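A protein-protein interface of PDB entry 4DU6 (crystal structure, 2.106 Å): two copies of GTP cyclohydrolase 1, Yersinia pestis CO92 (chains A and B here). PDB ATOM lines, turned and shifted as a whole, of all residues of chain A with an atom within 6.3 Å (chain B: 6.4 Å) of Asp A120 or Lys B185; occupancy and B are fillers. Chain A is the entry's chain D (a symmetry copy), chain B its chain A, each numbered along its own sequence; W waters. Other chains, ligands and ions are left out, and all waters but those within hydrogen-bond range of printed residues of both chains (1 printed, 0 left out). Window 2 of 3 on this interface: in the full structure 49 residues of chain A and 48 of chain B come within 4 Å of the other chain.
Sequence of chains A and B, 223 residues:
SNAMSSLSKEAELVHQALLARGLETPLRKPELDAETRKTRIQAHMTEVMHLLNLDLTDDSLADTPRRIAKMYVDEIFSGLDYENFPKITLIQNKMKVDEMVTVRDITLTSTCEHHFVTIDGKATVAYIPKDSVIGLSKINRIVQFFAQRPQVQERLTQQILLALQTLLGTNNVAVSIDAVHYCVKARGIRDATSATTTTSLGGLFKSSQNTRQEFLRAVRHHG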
ATOM      1  N   THR A 107       1.864  20.029  19.541  1.00  0.00           N
ATOM      2  CA  THR A 107       0.558  20.630  19.359  1.00  0.00           C
ATOM      3  C   THR A 107       0.561  21.611  18.185  1.00  0.00           C
ATOM      4  O   THR A 107       1.406  22.481  18.103  1.00  0.00           O
ATOM      5  CB  THR A 107       0.103  21.381  20.589  1.00  0.00           C
ATOM      6  OG1 THR A 107      -0.303  20.444  21.586  1.00  0.00           O
ATOM      7  CG2 THR A 107      -1.087  22.327  20.227  1.00  0.00           C
ATOM      8  N   LEU A 108      -0.370  21.431  17.256  1.00  0.00           N
ATOM      9  CA  LEU A 108      -0.417  22.249  16.049  1.00  0.00           C
ATOM     10  C   LEU A 108      -1.866  22.677  15.838  1.00  0.00           C
ATOM     11  O   LEU A 108      -2.795  21.847  15.811  1.00  0.00           O
ATOM     12  CB  LEU A 108       0.070  21.436  14.850  1.00  0.00           C
ATOM     13  CG  LEU A 108       0.335  22.127  13.521  1.00  0.00           C
ATOM     14  CD1 LEU A 108       1.374  21.323  12.753  1.00  0.00           C
ATOM     15  CD2 LEU A 108      -0.958  22.216  12.723  1.00  0.00           C
ATOM     16  N   THR A 109      -2.074  23.974  15.716  1.00  0.00           N
ATOM     17  CA  THR A 109      -3.402  24.475  15.386  1.00  0.00           C
ATOM     18  C   THR A 109      -3.220  25.495  14.272  1.00  0.00           C
ATOM     19  O   THR A 109      -2.351  26.366  14.352  1.00  0.00           O
ATOM     20  CB  THR A 109      -4.095  25.105  16.617  1.00  0.00           C
ATOM     21  OG1 THR A 109      -3.243  26.118  17.152  1.00  0.00           O
ATOM     22  CG2 THR A 109      -4.324  24.059  17.719  1.00  0.00           C
ATOM     23  N   SER A 110      -4.033  25.390  13.235  1.00  0.00           N
ATOM     24  CA  SER A 110      -3.847  26.170  12.030  1.00  0.00           C
ATOM     25  C   SER A 110      -5.166  26.506  11.378  1.00  0.00           C
ATOM     26  O   SER A 110      -6.221  26.164  11.889  1.00  0.00           O
ATOM     27  CB  SER A 110      -2.937  25.449  11.055  1.00  0.00           C
ATOM     28  OG  SER A 110      -2.623  26.282   9.968  1.00  0.00           O
ATOM     29  N   THR A 118     -10.725  26.167  11.332  1.00  0.00           N
ATOM     30  CA  THR A 118      -9.718  25.515  12.142  1.00  0.00           C
ATOM     31  C   THR A 118      -9.178  24.201  11.577  1.00  0.00           C
ATOM     32  O   THR A 118      -9.938  23.361  11.104  1.00  0.00           O
ATOM     33  CB  THR A 118     -10.330  25.197  13.496  1.00  0.00           C
ATOM     34  OG1 THR A 118     -10.602  26.428  14.171  1.00  0.00           O
ATOM     35  CG2 THR A 118      -9.395  24.344  14.320  1.00  0.00           C
ATOM     36  N   ILE A 119      -7.855  24.072  11.617  1.00  0.00           N
ATOM     37  CA  ILE A 119      -7.153  22.808  11.466  1.00  0.00           C
ATOM     38  C   ILE A 119      -6.555  22.433  12.820  1.00  0.00           C
ATOM     39  O   ILE A 119      -5.923  23.261  13.467  1.00  0.00           O
ATOM     40  CB  ILE A 119      -6.009  22.918  10.453  1.00  0.00           C
ATOM     41  CG1 ILE A 119      -6.558  23.210   9.054  1.00  0.00           C
ATOM     42  CG2 ILE A 119      -5.186  21.632  10.448  1.00  0.00           C
ATOM     43  CD1 ILE A 119      -5.492  23.668   8.082  1.00  0.00           C
ATOM     44  N   ASP A 120      -6.756  21.189  13.250  1.00  0.00           N
ATOM     45  CA  ASP A 120      -6.265  20.716  14.548  1.00  0.00           C
ATOM     46  C   ASP A 120      -5.412  19.474  14.330  1.00  0.00           C
ATOM     47  O   ASP A 120      -5.941  18.415  13.952  1.00  0.00           O
ATOM     48  CB  ASP A 120      -7.439  20.323  15.447  1.00  0.00           C
ATOM     49  CG  ASP A 120      -7.002  19.961  16.882  1.00  0.00           C
ATOM     50  OD1 ASP A 120      -5.966  20.457  17.337  1.00  0.00           O
ATOM     51  OD2 ASP A 120      -7.712  19.188  17.568  1.00  0.00           O
ATOM     52  N   GLY A 121      -4.113  19.583  14.606  1.00  0.00           N
ATOM     53  CA  GLY A 121      -3.175  18.508  14.339  1.00  0.00           C
ATOM     54  C   GLY A 121      -2.103  18.221  15.383  1.00  0.00           C
ATOM     55  O   GLY A 121      -2.086  18.822  16.461  1.00  0.00           O
ATOM     56  N   LYS A 122      -1.233  17.266  15.048  1.00  0.00           N
ATOM     57  CA  LYS A 122      -0.003  16.970  15.786  1.00  0.00           C
ATOM     58  C   LYS A 122       1.113  16.887  14.757  1.00  0.00           C
ATOM     59  O   LYS A 122       0.881  16.384  13.662  1.00  0.00           O
ATOM     60  CB  LYS A 122      -0.109  15.638  16.511  1.00  0.00           C
ATOM     61  CG  LYS A 122      -1.227  15.539  17.517  1.00  0.00           C
ATOM     62  CD  LYS A 122      -1.159  16.662  18.533  1.00  0.00           C
ATOM     63  CE  LYS A 122      -2.087  16.374  19.693  1.00  0.00           C
ATOM     64  NZ  LYS A 122      -1.772  15.029  20.264  1.00  0.00           N
ATOM     65  N   ASP A 178      -0.230  15.184  11.186  1.00  0.00           N
ATOM     66  CA  ASP A 178      -1.488  14.461  11.139  1.00  0.00           C
ATOM     67  C   ASP A 178      -2.568  15.394  11.685  1.00  0.00           C
ATOM     68  O   ASP A 178      -2.451  15.852  12.803  1.00  0.00           O
ATOM     69  CB  ASP A 178      -1.394  13.175  12.006  1.00  0.00           C
ATOM     70  CG  ASP A 178      -2.706  12.389  12.027  1.00  0.00           C
ATOM     71  OD1 ASP A 178      -3.026  11.732  11.010  1.00  0.00           O
ATOM     72  OD2 ASP A 178      -3.435  12.432  13.043  1.00  0.00           O
ATOM     73  N   ALA A 179      -3.606  15.686  10.909  1.00  0.00           N
ATOM     74  CA  ALA A 179      -4.557  16.732  11.297  1.00  0.00           C
ATOM     75  C   ALA A 179      -6.008  16.484  10.861  1.00  0.00           C
ATOM     76  O   ALA A 179      -6.256  15.806   9.866  1.00  0.00           O
ATOM     77  CB  ALA A 179      -4.102  18.079  10.763  1.00  0.00           C
ATOM     78  N   VAL A 180      -6.931  17.058  11.636  1.00  0.00           N
ATOM     79  CA  VAL A 180      -8.358  17.101  11.342  1.00  0.00           C
ATOM     80  C   VAL A 180      -8.664  18.497  10.811  1.00  0.00           C
ATOM     81  O   VAL A 180      -8.275  19.505  11.423  1.00  0.00           O
ATOM     82  CB  VAL A 180      -9.213  16.760  12.590  1.00  0.00           C
ATOM     83  CG1 VAL A 180     -10.666  17.107  12.392  1.00  0.00           C
ATOM     84  CG2 VAL A 180      -9.079  15.193  12.952  1.00  0.00           C
ATOM     85  N   HIS A 181      -9.266  18.529   9.626  1.00  0.00           N
ATOM     86  CA  HIS A 181      -9.678  19.751   8.950  1.00  0.00           C
ATOM     87  C   HIS A 181     -11.148  19.982   9.185  1.00  0.00           C
ATOM     88  O   HIS A 181     -11.992  19.191   8.745  1.00  0.00           O
ATOM     89  CB  HIS A 181      -9.431  19.622   7.460  1.00  0.00           C
ATOM     90  CG  HIS A 181      -7.984  19.653   7.095  1.00  0.00           C
ATOM     91  ND1 HIS A 181      -7.440  20.657   6.331  1.00  0.00           N
ATOM     92  CD2 HIS A 181      -6.962  18.833   7.426  1.00  0.00           C
ATOM     93  CE1 HIS A 181      -6.148  20.449   6.184  1.00  0.00           C
ATOM     94  NE2 HIS A 181      -5.829  19.341   6.828  1.00  0.00           N
ATOM     95  N   TYR A 182     -11.482  21.062   9.873  1.00  0.00           N
ATOM     96  CA  TYR A 182     -12.900  21.342  10.048  1.00  0.00           C
ATOM     97  C   TYR A 182     -13.659  21.770   8.774  1.00  0.00           C
ATOM     98  O   TYR A 182     -14.879  21.764   8.763  1.00  0.00           O
ATOM     99  CB  TYR A 182     -13.140  22.237  11.245  1.00  0.00           C
ATOM    100  CG  TYR A 182     -12.942  21.429  12.495  1.00  0.00           C
ATOM    101  CD1 TYR A 182     -11.693  21.345  13.098  1.00  0.00           C
ATOM    102  CD2 TYR A 182     -13.993  20.714  13.049  1.00  0.00           C
ATOM    103  CE1 TYR A 182     -11.510  20.623  14.227  1.00  0.00           C
ATOM    104  CE2 TYR A 182     -13.816  19.970  14.196  1.00  0.00           C
ATOM    105  CZ  TYR A 182     -12.560  19.918  14.769  1.00  0.00           C
ATOM    106  OH  TYR A 182     -12.353  19.195  15.903  1.00  0.00           O
ATOM    107  N   VAL B 180     -15.330  20.848  22.742  1.00  0.00           N
ATOM    108  CA  VAL B 180     -14.065  21.540  22.726  1.00  0.00           C
ATOM    109  C   VAL B 180     -14.275  22.857  21.979  1.00  0.00           C
ATOM    110  O   VAL B 180     -14.876  22.883  20.902  1.00  0.00           O
ATOM    111  CB  VAL B 180     -12.955  20.658  22.078  1.00  0.00           C
ATOM    112  CG1 VAL B 180     -11.698  21.487  21.731  1.00  0.00           C
ATOM    113  CG2 VAL B 180     -12.590  19.440  23.020  1.00  0.00           C
ATOM    114  N   HIS B 181     -13.855  23.958  22.591  1.00  0.00           N
ATOM    115  CA  HIS B 181     -13.962  25.297  21.953  1.00  0.00           C
ATOM    116  C   HIS B 181     -12.593  25.684  21.451  1.00  0.00           C
ATOM    117  O   HIS B 181     -11.634  25.799  22.238  1.00  0.00           O
ATOM    118  CB  HIS B 181     -14.437  26.355  22.953  1.00  0.00           C
ATOM    119  CG  HIS B 181     -15.851  26.159  23.399  1.00  0.00           C
ATOM    120  ND1 HIS B 181     -16.783  27.171  23.376  1.00  0.00           N
ATOM    121  CD2 HIS B 181     -16.499  25.067  23.867  1.00  0.00           C
ATOM    122  CE1 HIS B 181     -17.942  26.720  23.814  1.00  0.00           C
ATOM    123  NE2 HIS B 181     -17.802  25.441  24.108  1.00  0.00           N
ATOM    124  N   TYR B 182     -12.467  25.816  20.144  1.00  0.00           N
ATOM    125  CA  TYR B 182     -11.199  26.248  19.585  1.00  0.00           C
ATOM    126  C   TYR B 182     -10.780  27.701  19.921  1.00  0.00           C
ATOM    127  O   TYR B 182      -9.626  28.045  19.744  1.00  0.00           O
ATOM    128  CB  TYR B 182     -11.137  25.922  18.089  1.00  0.00           C
ATOM    129  CG  TYR B 182     -10.891  24.451  17.937  1.00  0.00           C
ATOM    130  CD1 TYR B 182     -11.951  23.564  17.826  1.00  0.00           C
ATOM    131  CD2 TYR B 182      -9.603  23.948  17.952  1.00  0.00           C
ATOM    132  CE1 TYR B 182     -11.737  22.230  17.711  1.00  0.00           C
ATOM    133  CE2 TYR B 182      -9.371  22.605  17.837  1.00  0.00           C
ATOM    134  CZ  TYR B 182     -10.451  21.747  17.728  1.00  0.00           C
ATOM    135  OH  TYR B 182     -10.251  20.405  17.617  1.00  0.00           O
ATOM    136  N   CYS B 183     -11.710  28.513  20.412  1.00  0.00           N
ATOM    137  CA  CYS B 183     -11.356  29.822  20.978  1.00  0.00           C
ATOM    138  C   CYS B 183     -10.679  29.701  22.347  1.00  0.00           C
ATOM    139  O   CYS B 183     -10.270  30.715  22.936  1.00  0.00           O
ATOM    140  CB  CYS B 183     -12.593  30.697  21.117  1.00  0.00           C
ATOM    141  SG  CYS B 183     -13.783  30.083  22.317  1.00  0.00           S
ATOM    142  N   VAL B 184     -10.602  28.466  22.858  1.00  0.00           N
ATOM    143  CA  VAL B 184      -9.865  28.135  24.068  1.00  0.00           C
ATOM    144  C   VAL B 184      -8.587  27.377  23.687  1.00  0.00           C
ATOM    145  O   VAL B 184      -7.509  27.615  24.248  1.00  0.00           O
ATOM    146  CB  VAL B 184     -10.742  27.253  25.001  1.00  0.00           C
ATOM    147  CG1 VAL B 184      -9.935  26.694  26.152  1.00  0.00           C
ATOM    148  CG2 VAL B 184     -11.960  28.039  25.479  1.00  0.00           C
ATOM    149  N   LYS B 185      -8.721  26.486  22.705  1.00  0.00           N
ATOM    150  CA  LYS B 185      -7.624  25.621  22.273  1.00  0.00           C
ATOM    151  C   LYS B 185      -6.671  26.275  21.248  1.00  0.00           C
ATOM    152  O   LYS B 185      -5.449  26.098  21.332  1.00  0.00           O
ATOM    153  CB  LYS B 185      -8.179  24.279  21.744  1.00  0.00           C
ATOM    154  CG  LYS B 185      -7.110  23.233  21.430  1.00  0.00           C
ATOM    155  CD  LYS B 185      -7.736  21.919  20.937  1.00  0.00           C
ATOM    156  CE  LYS B 185      -6.642  20.884  20.705  1.00  0.00           C
ATOM    157  NZ  LYS B 185      -7.213  19.506  20.615  1.00  0.00           N
ATOM    158  N   ALA B 186      -7.214  27.038  20.299  1.00  0.00           N
ATOM    159  CA  ALA B 186      -6.436  27.462  19.146  1.00  0.00           C
ATOM    160  C   ALA B 186      -5.897  28.906  19.269  1.00  0.00           C
ATOM    161  O   ALA B 186      -5.131  29.358  18.416  1.00  0.00           O
ATOM    162  CB  ALA B 186      -7.265  27.303  17.861  1.00  0.00           C
ATOM    163  N   ARG B 187      -6.320  29.619  20.313  1.00  0.00           N
ATOM    164  CA  ARG B 187      -5.927  31.033  20.534  1.00  0.00           C
ATOM    165  C   ARG B 187      -6.029  31.344  22.020  1.00  0.00           C
ATOM    166  O   ARG B 187      -6.501  30.521  22.820  1.00  0.00           O
ATOM    167  CB  ARG B 187      -6.846  31.957  19.760  1.00  0.00           C
ATOM    168  CG  ARG B 187      -8.296  31.609  19.992  1.00  0.00           C
ATOM    169  CD  ARG B 187      -9.147  32.835  20.041  1.00  0.00           C
ATOM    170  NE  ARG B 187      -8.533  33.963  20.721  1.00  0.00           N
ATOM    171  CZ  ARG B 187      -8.719  34.265  22.000  1.00  0.00           C
ATOM    172  NH1 ARG B 187      -8.127  35.344  22.509  1.00  0.00           N
ATOM    173  NH2 ARG B 187      -9.492  33.496  22.766  1.00  0.00           N
ATOM    174  N   ILE B 189      -5.436  31.468  25.743  1.00  0.00           N
ATOM    175  CA  ILE B 189      -4.747  30.578  26.659  1.00  0.00           C
ATOM    176  C   ILE B 189      -4.260  29.243  26.022  1.00  0.00           C
ATOM    177  O   ILE B 189      -3.326  28.630  26.517  1.00  0.00           O
ATOM    178  CB  ILE B 189      -5.592  30.307  27.879  1.00  0.00           C
ATOM    179  CG1 ILE B 189      -4.681  29.820  29.004  1.00  0.00           C
ATOM    180  CG2 ILE B 189      -6.764  29.365  27.512  1.00  0.00           C
ATOM    181  CD1 ILE B 189      -5.381  29.492  30.270  1.00  0.00           C
ATOM    182  N   ARG B 190      -4.864  28.825  24.917  1.00  0.00           N
ATOM    183  CA  ARG B 190      -4.397  27.647  24.165  1.00  0.00           C
ATOM    184  C   ARG B 190      -4.326  26.378  25.039  1.00  0.00           C
ATOM    185  O   ARG B 190      -3.282  25.708  25.141  1.00  0.00           O
ATOM    186  CB  ARG B 190      -3.058  27.918  23.457  1.00  0.00           C
ATOM    187  CG  ARG B 190      -3.159  28.941  22.317  1.00  0.00           C
ATOM    188  CD  ARG B 190      -1.809  29.264  21.700  1.00  0.00           C
ATOM    189  NE  ARG B 190      -1.914  30.364  20.732  1.00  0.00           N
ATOM    190  CZ  ARG B 190      -2.110  30.184  19.425  1.00  0.00           C
ATOM    191  NH1 ARG B 190      -2.204  28.937  18.943  1.00  0.00           N
ATOM    192  NH2 ARG B 190      -2.216  31.235  18.602  1.00  0.00           N
ATOM    193  N   ASP B 191      -5.444  26.081  25.694  1.00  0.00           N
ATOM    194  CA  ASP B 191      -5.558  24.847  26.467  1.00  0.00           C
ATOM    195  C   ASP B 191      -5.939  23.679  25.530  1.00  0.00           C
ATOM    196  O   ASP B 191      -7.062  23.617  25.028  1.00  0.00           O
ATOM    197  CB  ASP B 191      -6.577  25.002  27.597  1.00  0.00           C
ATOM    198  CG  ASP B 191      -6.520  23.833  28.599  1.00  0.00           C
ATOM    199  OD1 ASP B 191      -6.367  22.664  28.173  1.00  0.00           O
ATOM    200  OD2 ASP B 191      -6.630  24.099  29.808  1.00  0.00           O
ATOM    201  N   ALA B 192      -4.962  22.814  25.279  1.00  0.00           N
ATOM    202  CA  ALA B 192      -5.094  21.611  24.460  1.00  0.00           C
ATOM    203  C   ALA B 192      -5.998  20.513  25.056  1.00  0.00           C
ATOM    204  O   ALA B 192      -6.457  19.616  24.339  1.00  0.00           O
ATOM    205  CB  ALA B 192      -3.700  21.016  24.181  1.00  0.00           C
ATOM    206  N   THR B 193      -6.232  20.564  26.362  1.00  0.00           N
ATOM    207  CA  THR B 193      -6.871  19.426  27.030  1.00  0.00           C
ATOM    208  C   THR B 193      -8.313  19.650  27.439  1.00  0.00           C
ATOM    209  O   THR B 193      -9.042  18.696  27.587  1.00  0.00           O
ATOM    210  CB  THR B 193      -6.067  18.891  28.272  1.00  0.00           C
ATOM    211  OG1 THR B 193      -5.750  19.971  29.166  1.00  0.00           O
ATOM    212  CG2 THR B 193      -4.773  18.203  27.830  1.00  0.00           C
ATOM    213  N   SER B 194      -8.730  20.891  27.646  1.00  0.00           N
ATOM    214  CA  SER B 194      -9.982  21.108  28.355  1.00  0.00           C
ATOM    215  C   SER B 194     -11.221  20.922  27.479  1.00  0.00           C
ATOM    216  O   SER B 194     -11.132  20.950  26.251  1.00  0.00           O
ATOM    217  CB  SER B 194      -9.999  22.504  28.989  1.00  0.00           C
ATOM    218  OG  SER B 194     -10.281  23.484  28.023  1.00  0.00           O
HETATM  219  O   HOH W   1      -4.343  28.659  15.556  1.00  0.00           O
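The side-chain hydroxyl (OH) of Tyr B182 is in hydrogen-bond range of the side-chain carboxylate (OD2) of Asp A120. The side-chain hydroxyl (OH) of Tyr A182 sits at hydrogen-bond distance from the side-chain hydroxyl (OH) of Tyr B182 (3.0 Å). The side-chain carboxylate of Asp A120 is in salt-bridge range of the side-chain amino group of Lys B185 (3.1 Å). The guanidinium group (NH1) of Arg B190 lies within hydrogen-bond range of the side-chain hydroxyl (OG1) of Thr A109, 3.5 Å away.
O of Val B184 is in hydrogen-bond range of N of Arg B190 (3.0 Å). NH1 of Arg B190 lies within hydrogen-bond range of O of Ala B186 (3.0 Å). N of Tyr A182 sits at hydrogen-bond distance from O of Thr A118, 3.0 Å away. O of Asp A120 is in hydrogen-bond range of N of Val A180.
OG1 of Thr A109 touches O of Ala B186, at 3.96 Å. Tyr B182 touches Thr A118 (CD2 to CG2, 3.7 Å).
Printed residues of chain B within 4 Å of Thr A118: Tyr B182 (3.7 Å). Asp A120 touches just these residues of chain B: Tyr B182 (2.8 Å) and Lys B185 (3.1 Å). Of chain A, only Asp A120 comes within 4 Å of Lys B185. Of the printed residues of chain A, Arg B190 touches Thr A109. The nearest residue of chain B that does not touch Asp A120 is Val B180 (6.2 Å). The nearest residue of chain A that does not touch Lys B185 is Thr A109 (4.3 Å).
Hydrophobic or aromatic side chains of chain A that line the printed part of chain B: Tyr A182. Of the 14 printed residues of chain B, 4 touch a printed residue of chain A. Among the printed residues, Asp or Glu carboxylates within 4 Å of a Lys or Arg side-chain nitrogen of the other chain: Asp A120 with Lys B185.
Tyr B182 touches its own counterpart, Tyr A182. Positions printed for both chains: 180, 181 and 182.
Water W1 lies within hydrogen-bond range of the backbone carbonyl oxygen of Ala B186 and the side-chain hydroxyl of Thr A109.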
